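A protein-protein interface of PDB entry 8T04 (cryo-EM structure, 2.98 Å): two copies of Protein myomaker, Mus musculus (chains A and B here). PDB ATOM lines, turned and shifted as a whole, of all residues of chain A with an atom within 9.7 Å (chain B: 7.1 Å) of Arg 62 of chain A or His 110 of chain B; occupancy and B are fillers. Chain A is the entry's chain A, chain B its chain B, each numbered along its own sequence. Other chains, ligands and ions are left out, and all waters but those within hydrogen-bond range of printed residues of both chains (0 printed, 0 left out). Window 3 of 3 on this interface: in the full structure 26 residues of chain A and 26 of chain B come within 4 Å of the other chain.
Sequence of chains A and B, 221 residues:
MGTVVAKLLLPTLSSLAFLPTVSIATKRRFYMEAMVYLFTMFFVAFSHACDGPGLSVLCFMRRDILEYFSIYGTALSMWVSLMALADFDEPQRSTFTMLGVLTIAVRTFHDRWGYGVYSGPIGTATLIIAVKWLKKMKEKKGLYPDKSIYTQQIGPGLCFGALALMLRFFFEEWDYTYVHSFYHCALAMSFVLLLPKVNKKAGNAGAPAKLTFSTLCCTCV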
ATOM      1  N   PHE A  43     -21.775 -16.563  -3.079  1.00  0.00           N
ATOM      2  CA  PHE A  43     -21.740 -15.451  -2.090  1.00  0.00           C
ATOM      3  C   PHE A  43     -21.993 -15.979  -0.671  1.00  0.00           C
ATOM      4  O   PHE A  43     -21.401 -15.403   0.256  1.00  0.00           O
ATOM      5  CB  PHE A  43     -22.686 -14.317  -2.496  1.00  0.00           C
ATOM      6  CG  PHE A  43     -22.072 -13.363  -3.489  1.00  0.00           C
ATOM      7  CD1 PHE A  43     -21.086 -12.472  -3.089  1.00  0.00           C
ATOM      8  CD2 PHE A  43     -22.447 -13.375  -4.824  1.00  0.00           C
ATOM      9  CE1 PHE A  43     -20.503 -11.602  -3.997  1.00  0.00           C
ATOM     10  CE2 PHE A  43     -21.863 -12.503  -5.732  1.00  0.00           C
ATOM     11  CZ  PHE A  43     -20.892 -11.618  -5.317  1.00  0.00           C
ATOM     12  N   PHE A  46     -18.595 -17.880   0.287  1.00  0.00           N
ATOM     13  CA  PHE A  46     -17.512 -16.889   0.534  1.00  0.00           C
ATOM     14  C   PHE A  46     -17.861 -15.996   1.731  1.00  0.00           C
ATOM     15  O   PHE A  46     -16.908 -15.555   2.393  1.00  0.00           O
ATOM     16  CB  PHE A  46     -17.177 -16.096  -0.734  1.00  0.00           C
ATOM     17  CG  PHE A  46     -16.123 -16.765  -1.578  1.00  0.00           C
ATOM     18  CD1 PHE A  46     -16.455 -17.794  -2.448  1.00  0.00           C
ATOM     19  CD2 PHE A  46     -14.787 -16.405  -1.463  1.00  0.00           C
ATOM     20  CE1 PHE A  46     -15.482 -18.425  -3.207  1.00  0.00           C
ATOM     21  CE2 PHE A  46     -13.814 -17.038  -2.222  1.00  0.00           C
ATOM     22  CZ  PHE A  46     -14.163 -18.047  -3.093  1.00  0.00           C
ATOM     23  N   SER A  47     -19.146 -15.747   2.014  1.00  0.00           N
ATOM     24  CA  SER A  47     -19.595 -15.007   3.226  1.00  0.00           C
ATOM     25  C   SER A  47     -19.148 -15.755   4.490  1.00  0.00           C
ATOM     26  O   SER A  47     -18.669 -15.084   5.426  1.00  0.00           O
ATOM     27  CB  SER A  47     -21.084 -14.771   3.233  1.00  0.00           C
ATOM     28  OG  SER A  47     -21.485 -14.084   4.409  1.00  0.00           O
ATOM     29  N   CYS A  50     -15.031 -16.102   4.511  1.00  0.00           N
ATOM     30  CA  CYS A  50     -14.449 -14.770   4.840  1.00  0.00           C
ATOM     31  C   CYS A  50     -14.688 -14.427   6.319  1.00  0.00           C
ATOM     32  O   CYS A  50     -13.837 -13.725   6.900  1.00  0.00           O
ATOM     33  CB  CYS A  50     -15.013 -13.681   3.932  1.00  0.00           C
ATOM     34  SG  CYS A  50     -13.970 -12.200   3.836  1.00  0.00           S
ATOM     35  N   ASP A  51     -15.797 -14.904   6.898  1.00  0.00           N
ATOM     36  CA  ASP A  51     -16.165 -14.716   8.329  1.00  0.00           C
ATOM     37  C   ASP A  51     -15.288 -15.606   9.226  1.00  0.00           C
ATOM     38  O   ASP A  51     -14.936 -15.148  10.331  1.00  0.00           O
ATOM     39  CB  ASP A  51     -17.656 -14.998   8.547  1.00  0.00           C
ATOM     40  CG  ASP A  51     -18.143 -14.735   9.962  1.00  0.00           C
ATOM     41  OD1 ASP A  51     -18.015 -13.582  10.420  1.00  0.00           O
ATOM     42  OD2 ASP A  51     -18.644 -15.686  10.597  1.00  0.00           O
ATOM     43  N   SER A  56     -10.181 -17.107   6.451  1.00  0.00           N
ATOM     44  CA  SER A  56     -10.546 -15.742   5.972  1.00  0.00           C
ATOM     45  C   SER A  56      -9.558 -15.228   4.911  1.00  0.00           C
ATOM     46  O   SER A  56      -9.919 -14.269   4.201  1.00  0.00           O
ATOM     47  CB  SER A  56     -10.633 -14.770   7.121  1.00  0.00           C
ATOM     48  OG  SER A  56     -11.125 -13.511   6.688  1.00  0.00           O
ATOM     49  N   CYS A  59     -10.802 -15.050   0.992  1.00  0.00           N
ATOM     50  CA  CYS A  59     -11.712 -14.009   0.428  1.00  0.00           C
ATOM     51  C   CYS A  59     -10.920 -12.782  -0.044  1.00  0.00           C
ATOM     52  O   CYS A  59      -9.828 -12.523   0.505  1.00  0.00           O
ATOM     53  CB  CYS A  59     -12.821 -13.618   1.400  1.00  0.00           C
ATOM     54  SG  CYS A  59     -12.253 -12.801   2.913  1.00  0.00           S
ATOM     55  N   PHE A  60     -11.480 -12.064  -1.026  1.00  0.00           N
ATOM     56  CA  PHE A  60     -10.809 -11.011  -1.839  1.00  0.00           C
ATOM     57  C   PHE A  60     -11.648  -9.724  -1.860  1.00  0.00           C
ATOM     58  O   PHE A  60     -11.051  -8.638  -1.706  1.00  0.00           O
ATOM     59  CB  PHE A  60     -10.503 -11.537  -3.245  1.00  0.00           C
ATOM     60  CG  PHE A  60     -11.665 -12.153  -3.987  1.00  0.00           C
ATOM     61  CD1 PHE A  60     -12.031 -13.474  -3.767  1.00  0.00           C
ATOM     62  CD2 PHE A  60     -12.380 -11.419  -4.922  1.00  0.00           C
ATOM     63  CE1 PHE A  60     -13.096 -14.041  -4.454  1.00  0.00           C
ATOM     64  CE2 PHE A  60     -13.443 -11.987  -5.610  1.00  0.00           C
ATOM     65  CZ  PHE A  60     -13.799 -13.297  -5.374  1.00  0.00           C
ATOM     66  N   MET A  61     -12.969  -9.828  -2.052  1.00  0.00           N
ATOM     67  CA  MET A  61     -13.924  -8.705  -1.852  1.00  0.00           C
ATOM     68  C   MET A  61     -14.066  -8.440  -0.348  1.00  0.00           C
ATOM     69  O   MET A  61     -13.814  -9.366   0.451  1.00  0.00           O
ATOM     70  CB  MET A  61     -15.298  -9.007  -2.463  1.00  0.00           C
ATOM     71  CG  MET A  61     -15.311  -8.901  -3.979  1.00  0.00           C
ATOM     72  SD  MET A  61     -16.929  -9.249  -4.718  1.00  0.00           S
ATOM     73  CE  MET A  61     -16.961 -11.038  -4.625  1.00  0.00           C
ATOM     74  N   ARG A  62     -14.448  -7.209   0.003  1.00  0.00           N
ATOM     75  CA  ARG A  62     -14.750  -6.743   1.387  1.00  0.00           C
ATOM     76  C   ARG A  62     -15.843  -7.634   1.994  1.00  0.00           C
ATOM     77  O   ARG A  62     -16.655  -8.182   1.217  1.00  0.00           O
ATOM     78  CB  ARG A  62     -15.251  -5.297   1.340  1.00  0.00           C
ATOM     79  CG  ARG A  62     -14.259  -4.286   0.775  1.00  0.00           C
ATOM     80  CD  ARG A  62     -14.850  -2.929   0.410  1.00  0.00           C
ATOM     81  NE  ARG A  62     -16.296  -2.918   0.176  1.00  0.00           N
ATOM     82  CZ  ARG A  62     -16.956  -2.145  -0.690  1.00  0.00           C
ATOM     83  NH1 ARG A  62     -16.325  -1.289  -1.480  1.00  0.00           N
ATOM     84  NH2 ARG A  62     -18.272  -2.256  -0.776  1.00  0.00           N
ATOM     85  N   ARG A  63     -15.878  -7.754   3.326  1.00  0.00           N
ATOM     86  CA  ARG A  63     -16.908  -8.532   4.076  1.00  0.00           C
ATOM     87  C   ARG A  63     -18.310  -7.984   3.792  1.00  0.00           C
ATOM     88  O   ARG A  63     -19.265  -8.789   3.777  1.00  0.00           O
ATOM     89  CB  ARG A  63     -16.647  -8.486   5.585  1.00  0.00           C
ATOM     90  CG  ARG A  63     -15.697  -9.569   6.076  1.00  0.00           C
ATOM     91  CD  ARG A  63     -15.981 -10.024   7.497  1.00  0.00           C
ATOM     92  NE  ARG A  63     -17.409 -10.146   7.783  1.00  0.00           N
ATOM     93  CZ  ARG A  63     -18.218 -11.111   7.338  1.00  0.00           C
ATOM     94  NH1 ARG A  63     -17.761 -12.092   6.573  1.00  0.00           N
ATOM     95  NH2 ARG A  63     -19.500 -11.092   7.667  1.00  0.00           N
ATOM     96  N   ASP A  64     -18.415  -6.667   3.596  1.00  0.00           N
ATOM     97  CA  ASP A  64     -19.681  -5.924   3.362  1.00  0.00           C
ATOM     98  C   ASP A  64     -20.363  -6.420   2.079  1.00  0.00           C
ATOM     99  O   ASP A  64     -21.601  -6.578   2.104  1.00  0.00           O
ATOM    100  CB  ASP A  64     -19.399  -4.419   3.312  1.00  0.00           C
ATOM    101  CG  ASP A  64     -20.636  -3.545   3.193  1.00  0.00           C
ATOM    102  OD1 ASP A  64     -21.696  -3.946   3.715  1.00  0.00           O
ATOM    103  OD2 ASP A  64     -20.529  -2.465   2.579  1.00  0.00           O
ATOM    104  N   ILE A  65     -19.593  -6.656   1.008  1.00  0.00           N
ATOM    105  CA  ILE A  65     -20.115  -7.089  -0.326  1.00  0.00           C
ATOM    106  C   ILE A  65     -20.625  -8.531  -0.200  1.00  0.00           C
ATOM    107  O   ILE A  65     -21.761  -8.791  -0.640  1.00  0.00           O
ATOM    108  CB  ILE A  65     -19.051  -6.943  -1.440  1.00  0.00           C
ATOM    109  CG1 ILE A  65     -18.526  -5.506  -1.548  1.00  0.00           C
ATOM    110  CG2 ILE A  65     -19.599  -7.438  -2.776  1.00  0.00           C
ATOM    111  CD1 ILE A  65     -17.340  -5.336  -2.474  1.00  0.00           C
ATOM    112  N   LEU A  66     -19.817  -9.416   0.393  1.00  0.00           N
ATOM    113  CA  LEU A  66     -20.111 -10.870   0.536  1.00  0.00           C
ATOM    114  C   LEU A  66     -21.356 -11.070   1.406  1.00  0.00           C
ATOM    115  O   LEU A  66     -22.194 -11.917   1.046  1.00  0.00           O
ATOM    116  CB  LEU A  66     -18.895 -11.577   1.145  1.00  0.00           C
ATOM    117  CG  LEU A  66     -17.623 -11.561   0.297  1.00  0.00           C
ATOM    118  CD1 LEU A  66     -16.459 -12.162   1.066  1.00  0.00           C
ATOM    119  CD2 LEU A  66     -17.823 -12.294  -1.021  1.00  0.00           C
ATOM    120  N   GLU A  67     -21.463 -10.309   2.500  1.00  0.00           N
ATOM    121  CA  GLU A  67     -22.593 -10.347   3.466  1.00  0.00           C
ATOM    122  C   GLU A  67     -23.882  -9.855   2.794  1.00  0.00           C
ATOM    123  O   GLU A  67     -24.935 -10.477   3.041  1.00  0.00           O
ATOM    124  CB  GLU A  67     -22.243  -9.505   4.692  1.00  0.00           C
ATOM    125  CG  GLU A  67     -23.338  -9.430   5.738  1.00  0.00           C
ATOM    126  CD  GLU A  67     -22.932  -8.621   6.957  1.00  0.00           C
ATOM    127  OE1 GLU A  67     -22.100  -9.119   7.741  1.00  0.00           O
ATOM    128  OE2 GLU A  67     -23.440  -7.491   7.113  1.00  0.00           O
ATOM    129  N   TYR A  68     -23.814  -8.772   2.008  1.00  0.00           N
ATOM    130  CA  TYR A  68     -24.986  -8.180   1.309  1.00  0.00           C
ATOM    131  C   TYR A  68     -25.539  -9.180   0.283  1.00  0.00           C
ATOM    132  O   TYR A  68     -26.764  -9.416   0.293  1.00  0.00           O
ATOM    133  CB  TYR A  68     -24.649  -6.840   0.645  1.00  0.00           C
ATOM    134  CG  TYR A  68     -25.779  -6.293  -0.192  1.00  0.00           C
ATOM    135  CD1 TYR A  68     -26.925  -5.785   0.400  1.00  0.00           C
ATOM    136  CD2 TYR A  68     -25.729  -6.330  -1.578  1.00  0.00           C
ATOM    137  CE1 TYR A  68     -27.978  -5.304  -0.361  1.00  0.00           C
ATOM    138  CE2 TYR A  68     -26.775  -5.852  -2.353  1.00  0.00           C
ATOM    139  CZ  TYR A  68     -27.904  -5.336  -1.743  1.00  0.00           C
ATOM    140  OH  TYR A  68     -28.936  -4.861  -2.501  1.00  0.00           O
ATOM    141  N   PHE A  69     -24.672  -9.747  -0.564  1.00  0.00           N
ATOM    142  CA  PHE A  69     -25.056 -10.628  -1.703  1.00  0.00           C
ATOM    143  C   PHE A  69     -25.287 -12.070  -1.231  1.00  0.00           C
ATOM    144  O   PHE A  69     -25.873 -12.851  -2.007  1.00  0.00           O
ATOM    145  CB  PHE A  69     -24.029 -10.533  -2.833  1.00  0.00           C
ATOM    146  CG  PHE A  69     -24.128  -9.222  -3.568  1.00  0.00           C
ATOM    147  CD1 PHE A  69     -25.286  -8.900  -4.260  1.00  0.00           C
ATOM    148  CD2 PHE A  69     -23.106  -8.288  -3.518  1.00  0.00           C
ATOM    149  CE1 PHE A  69     -25.407  -7.686  -4.916  1.00  0.00           C
ATOM    150  CE2 PHE A  69     -23.227  -7.072  -4.173  1.00  0.00           C
ATOM    151  CZ  PHE A  69     -24.379  -6.772  -4.867  1.00  0.00           C
ATOM    152  N   SER A  70     -24.848 -12.410  -0.016  1.00  0.00           N
ATOM    153  CA  SER A  70     -25.282 -13.628   0.719  1.00  0.00           C
ATOM    154  C   SER A  70     -26.780 -13.519   1.028  1.00  0.00           C
ATOM    155  O   SER A  70     -27.525 -14.451   0.673  1.00  0.00           O
ATOM    156  CB  SER A  70     -24.473 -13.831   1.977  1.00  0.00           C
ATOM    157  OG  SER A  70     -25.044 -14.839   2.799  1.00  0.00           O
ATOM    158  N   PHE A 109     -30.864  -3.516   0.795  1.00  0.00           N
ATOM    159  CA  PHE A 109     -29.871  -2.407   0.787  1.00  0.00           C
ATOM    160  C   PHE A 109     -30.194  -1.410   1.907  1.00  0.00           C
ATOM    161  O   PHE A 109     -29.248  -0.951   2.578  1.00  0.00           O
ATOM    162  CB  PHE A 109     -29.817  -1.718  -0.580  1.00  0.00           C
ATOM    163  CG  PHE A 109     -28.693  -0.724  -0.717  1.00  0.00           C
ATOM    164  CD1 PHE A 109     -28.831   0.574  -0.247  1.00  0.00           C
ATOM    165  CD2 PHE A 109     -27.485  -1.092  -1.296  1.00  0.00           C
ATOM    166  CE1 PHE A 109     -27.790   1.484  -0.358  1.00  0.00           C
ATOM    167  CE2 PHE A 109     -26.447  -0.179  -1.410  1.00  0.00           C
ATOM    168  CZ  PHE A 109     -26.602   1.107  -0.942  1.00  0.00           C
ATOM    169  N   ARG A 112     -30.453  -4.868   5.807  1.00  0.00           N
ATOM    170  CA  ARG A 112     -30.257  -6.295   5.428  1.00  0.00           C
ATOM    171  C   ARG A 112     -30.628  -7.227   6.593  1.00  0.00           C
ATOM    172  O   ARG A 112     -30.777  -8.438   6.332  1.00  0.00           O
ATOM    173  CB  ARG A 112     -28.825  -6.550   4.939  1.00  0.00           C
ATOM    174  CG  ARG A 112     -27.730  -6.325   5.973  1.00  0.00           C
ATOM    175  CD  ARG A 112     -26.350  -6.370   5.348  1.00  0.00           C
ATOM    176  NE  ARG A 112     -26.071  -5.219   4.493  1.00  0.00           N
ATOM    177  CZ  ARG A 112     -24.871  -4.868   4.033  1.00  0.00           C
ATOM    178  NH1 ARG A 112     -23.789  -5.568   4.341  1.00  0.00           N
ATOM    179  NH2 ARG A 112     -24.752  -3.801   3.259  1.00  0.00           N
ATOM    180  N   TYR B  68     -27.383   5.224  -4.889  1.00  0.00           N
ATOM    181  CA  TYR B  68     -27.071   3.842  -5.345  1.00  0.00           C
ATOM    182  C   TYR B  68     -28.081   3.405  -6.416  1.00  0.00           C
ATOM    183  O   TYR B  68     -27.639   2.915  -7.475  1.00  0.00           O
ATOM    184  CB  TYR B  68     -27.036   2.841  -4.185  1.00  0.00           C
ATOM    185  CG  TYR B  68     -26.869   1.413  -4.640  1.00  0.00           C
ATOM    186  CD1 TYR B  68     -25.659   0.962  -5.144  1.00  0.00           C
ATOM    187  CD2 TYR B  68     -27.932   0.523  -4.615  1.00  0.00           C
ATOM    188  CE1 TYR B  68     -25.503  -0.342  -5.589  1.00  0.00           C
ATOM    189  CE2 TYR B  68     -27.791  -0.784  -5.056  1.00  0.00           C
ATOM    190  CZ  TYR B  68     -26.572  -1.220  -5.545  1.00  0.00           C
ATOM    191  OH  TYR B  68     -26.428  -2.506  -5.976  1.00  0.00           O
ATOM    192  N   ILE B 104     -24.503  -6.215 -12.714  1.00  0.00           N
ATOM    193  CA  ILE B 104     -24.606  -4.733 -12.516  1.00  0.00           C
ATOM    194  C   ILE B 104     -24.805  -4.445 -11.020  1.00  0.00           C
ATOM    195  O   ILE B 104     -24.229  -3.446 -10.547  1.00  0.00           O
ATOM    196  CB  ILE B 104     -25.709  -4.106 -13.402  1.00  0.00           C
ATOM    197  CG1 ILE B 104     -25.372  -4.259 -14.889  1.00  0.00           C
ATOM    198  CG2 ILE B 104     -25.952  -2.643 -13.044  1.00  0.00           C
ATOM    199  CD1 ILE B 104     -26.524  -3.976 -15.829  1.00  0.00           C
ATOM    200  N   ALA B 105     -25.577  -5.278 -10.310  1.00  0.00           N
ATOM    201  CA  ALA B 105     -25.822  -5.165  -8.851  1.00  0.00           C
ATOM    202  C   ALA B 105     -24.486  -5.216  -8.101  1.00  0.00           C
ATOM    203  O   ALA B 105     -24.217  -4.276  -7.329  1.00  0.00           O
ATOM    204  CB  ALA B 105     -26.758  -6.249  -8.377  1.00  0.00           C
ATOM    205  N   VAL B 106     -23.677  -6.255  -8.347  1.00  0.00           N
ATOM    206  CA  VAL B 106     -22.358  -6.476  -7.676  1.00  0.00           C
ATOM    207  C   VAL B 106     -21.396  -5.361  -8.089  1.00  0.00           C
ATOM    208  O   VAL B 106     -20.688  -4.848  -7.196  1.00  0.00           O
ATOM    209  CB  VAL B 106     -21.754  -7.863  -7.979  1.00  0.00           C
ATOM    210  CG1 VAL B 106     -20.353  -8.016  -7.397  1.00  0.00           C
ATOM    211  CG2 VAL B 106     -22.646  -8.984  -7.476  1.00  0.00           C
ATOM    212  N   ARG B 107     -21.352  -5.021  -9.379  1.00  0.00           N
ATOM    213  CA  ARG B 107     -20.397  -4.007  -9.892  1.00  0.00           C
ATOM    214  C   ARG B 107     -20.680  -2.661  -9.217  1.00  0.00           C
ATOM    215  O   ARG B 107     -19.731  -2.076  -8.656  1.00  0.00           O
ATOM    216  CB  ARG B 107     -20.458  -3.862 -11.416  1.00  0.00           C
ATOM    217  CG  ARG B 107     -19.554  -2.761 -11.957  1.00  0.00           C
ATOM    218  CD  ARG B 107     -18.112  -2.953 -11.516  1.00  0.00           C
ATOM    219  NE  ARG B 107     -17.229  -1.837 -11.830  1.00  0.00           N
ATOM    220  CZ  ARG B 107     -16.340  -1.281 -10.998  1.00  0.00           C
ATOM    221  NH1 ARG B 107     -16.175  -1.723  -9.759  1.00  0.00           N
ATOM    222  NH2 ARG B 107     -15.599  -0.273 -11.419  1.00  0.00           N
ATOM    223  N   THR B 108     -21.933  -2.197  -9.282  1.00  0.00           N
ATOM    224  CA  THR B 108     -22.380  -0.888  -8.730  1.00  0.00           C
ATOM    225  C   THR B 108     -22.190  -0.862  -7.207  1.00  0.00           C
ATOM    226  O   THR B 108     -21.802   0.204  -6.696  1.00  0.00           O
ATOM    227  CB  THR B 108     -23.832  -0.567  -9.109  1.00  0.00           C
ATOM    228  OG1 THR B 108     -24.018  -0.853 -10.495  1.00  0.00           O
ATOM    229  CG2 THR B 108     -24.191   0.880  -8.847  1.00  0.00           C
ATOM    230  N   PHE B 109     -22.452  -1.976  -6.514  1.00  0.00           N
ATOM    231  CA  PHE B 109     -22.349  -2.081  -5.034  1.00  0.00           C
ATOM    232  C   PHE B 109     -20.876  -2.023  -4.608  1.00  0.00           C
ATOM    233  O   PHE B 109     -20.580  -1.346  -3.603  1.00  0.00           O
ATOM    234  CB  PHE B 109     -23.035  -3.349  -4.515  1.00  0.00           C
ATOM    235  CG  PHE B 109     -23.144  -3.408  -3.013  1.00  0.00           C
ATOM    236  CD1 PHE B 109     -22.082  -3.856  -2.241  1.00  0.00           C
ATOM    237  CD2 PHE B 109     -24.300  -2.993  -2.367  1.00  0.00           C
ATOM    238  CE1 PHE B 109     -22.175  -3.897  -0.858  1.00  0.00           C
ATOM    239  CE2 PHE B 109     -24.395  -3.037  -0.984  1.00  0.00           C
ATOM    240  CZ  PHE B 109     -23.333  -3.489  -0.231  1.00  0.00           C
ATOM    241  N   HIS B 110     -19.998  -2.728  -5.333  1.00  0.00           N
ATOM    242  CA  HIS B 110     -18.524  -2.745  -5.120  1.00  0.00           C
ATOM    243  C   HIS B 110     -17.971  -1.317  -5.221  1.00  0.00           C
ATOM    244  O   HIS B 110     -17.293  -0.878  -4.270  1.00  0.00           O
ATOM    245  CB  HIS B 110     -17.842  -3.702  -6.110  1.00  0.00           C
ATOM    246  CG  HIS B 110     -16.354  -3.585  -6.136  1.00  0.00           C
ATOM    247  ND1 HIS B 110     -15.631  -3.618  -7.313  1.00  0.00           N
ATOM    248  CD2 HIS B 110     -15.455  -3.411  -5.144  1.00  0.00           C
ATOM    249  CE1 HIS B 110     -14.349  -3.483  -7.042  1.00  0.00           C
ATOM    250  NE2 HIS B 110     -14.214  -3.351  -5.717  1.00  0.00           N
ATOM    251  N   ASP B 111     -18.250  -0.637  -6.336  1.00  0.00           N
ATOM    252  CA  ASP B 111     -17.842   0.771  -6.594  1.00  0.00           C
ATOM    253  C   ASP B 111     -18.812   1.379  -7.613  1.00  0.00           C
ATOM    254  O   ASP B 111     -18.787   0.947  -8.784  1.00  0.00           O
ATOM    255  CB  ASP B 111     -16.386   0.845  -7.068  1.00  0.00           C
ATOM    256  CG  ASP B 111     -15.794   2.246  -7.111  1.00  0.00           C
ATOM    257  OD1 ASP B 111     -16.566   3.228  -7.062  1.00  0.00           O
ATOM    258  OD2 ASP B 111     -14.552   2.346  -7.191  1.00  0.00           O
ATOM    259  N   ARG B 112     -19.625   2.345  -7.175  1.00  0.00           N
ATOM    260  CA  ARG B 112     -20.709   2.956  -7.994  1.00  0.00           C
ATOM    261  C   ARG B 112     -20.150   4.059  -8.906  1.00  0.00           C
ATOM    262  O   ARG B 112     -20.886   4.464  -9.829  1.00  0.00           O
ATOM    263  CB  ARG B 112     -21.843   3.484  -7.107  1.00  0.00           C
ATOM    264  CG  ARG B 112     -21.464   4.614  -6.159  1.00  0.00           C
ATOM    265  CD  ARG B 112     -22.570   4.910  -5.167  1.00  0.00           C
ATOM    266  NE  ARG B 112     -22.748   3.851  -4.177  1.00  0.00           N
ATOM    267  CZ  ARG B 112     -23.456   3.955  -3.050  1.00  0.00           C
ATOM    268  NH1 ARG B 112     -24.070   5.085  -2.732  1.00  0.00           N
ATOM    269  NH2 ARG B 112     -23.543   2.918  -2.234  1.00  0.00           N
ATOM    270  N   TRP B 113     -18.917   4.526  -8.666  1.00  0.00           N
ATOM    271  CA  TRP B 113     -18.249   5.612  -9.437  1.00  0.00           C
ATOM    272  C   TRP B 113     -17.055   5.094 -10.251  1.00  0.00           C
ATOM    273  O   TRP B 113     -16.459   5.917 -10.959  1.00  0.00           O
ATOM    274  CB  TRP B 113     -17.770   6.727  -8.502  1.00  0.00           C
ATOM    275  CG  TRP B 113     -18.804   7.323  -7.600  1.00  0.00           C
ATOM    276  CD1 TRP B 113     -18.800   7.285  -6.237  1.00  0.00           C
ATOM    277  CD2 TRP B 113     -19.960   8.094  -7.978  1.00  0.00           C
ATOM    278  NE1 TRP B 113     -19.878   7.961  -5.738  1.00  0.00           N
ATOM    279  CE2 TRP B 113     -20.608   8.468  -6.780  1.00  0.00           C
ATOM    280  CE3 TRP B 113     -20.520   8.497  -9.199  1.00  0.00           C
ATOM    281  CZ2 TRP B 113     -21.783   9.221  -6.773  1.00  0.00           C
ATOM    282  CZ3 TRP B 113     -21.682   9.243  -9.189  1.00  0.00           C
ATOM    283  CH2 TRP B 113     -22.302   9.600  -7.990  1.00  0.00           C
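Hydrophobic or aromatic side chains of chain B that line the printed part of chain A: Tyr 68, Ala 105, Val 106, Phe 109 and His 110.
Of the 20 printed residues of chain A, 7 touch a printed residue of chain B.
Along chain A the printed residues that touch a printed residue of chain B span positions 43 to 112.
The side-chain carboxylate of Asp 64 of chain A is in salt-bridge range of the guanidinium group of Arg 112 of chain A, at 2.7 Å.
The guanidinium group (NH1) of Arg 112 of chain A lies within salt-bridge range of the side-chain carboxylate (OE2) of Glu 67 of chain A, at 3.4 Å.
O of Ala 105 of chain B lies within hydrogen-bond range of OH of Tyr 68 of chain B.
The guanidinium group (NH1) of Arg 107 of chain B is in hydrogen-bond range of a ring nitrogen (ND1) of His 110 of chain B (3.1 Å).
SG of Cys 50 of chain A forms a disulfide with SG of Cys 59 of chain A (2.0 Å).
Among the printed residues, merely in contact across the chains: Phe 69 of chain A with Val 106 of chain B (3.5 Å), Phe 69 of chain A with Ala 105 of chain B (3.5 Å), Phe 109 of chain A with Phe 109 of chain B (3.5 Å), Phe 109 of chain A with Tyr 68 of chain B (3.6 Å), Tyr 68 of chain A with Phe 109 of chain B (3.6 Å), Phe 69 of chain A with Phe 109 of chain B (3.7 Å), Arg 62 of chain A with Phe 109 of chain B (3.8 Å), Arg 112 of chain A with Phe 109 of chain B (3.8 Å), Phe 109 of chain A with Arg 112 of chain B (3.8 Å), Ile 65 of chain A with His 110 of chain B (3.8 Å), Phe 43 of chain A with Val 106 of chain B (3.8 Å) and Ile 65 of chain A with Phe 109 of chain B (3.8 Å).
Tyr 68 of chain A touches Phe 109 of chain B, and with the chains exchanged Phe 109 of chain A touches Tyr 68 of chain B.
Phe 109 of chain A touches its own counterpart, Phe 109 of chain B.
Phe 109 of chain A touches Arg 112 of chain B, and with the chains exchanged Arg 112 of chain A touches Phe 109 of chain B.
3 positions are printed for both chains.
The guanidinium group (NH1) of Arg 62 of chain A sits at hydrogen-bond distance from the backbone carbonyl oxygen (O) of His 110 of chain B (3.0 Å).
Of the printed residues of chain B, Ile 65 of chain A touches Phe 109 and His 110.
Of the printed residues of chain B, Phe 69 of chain A touches Ala 105, Val 106 and Phe 109.
Of the printed residues of chain A, Tyr 68 of chain B touches Phe 109.
No residue of chain A comes within 4 Å of Asp 111 of chain B.
The nearest printed residue of chain B that does not touch Phe 43 of chain A is Arg 107 of chain B (7.8 Å).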
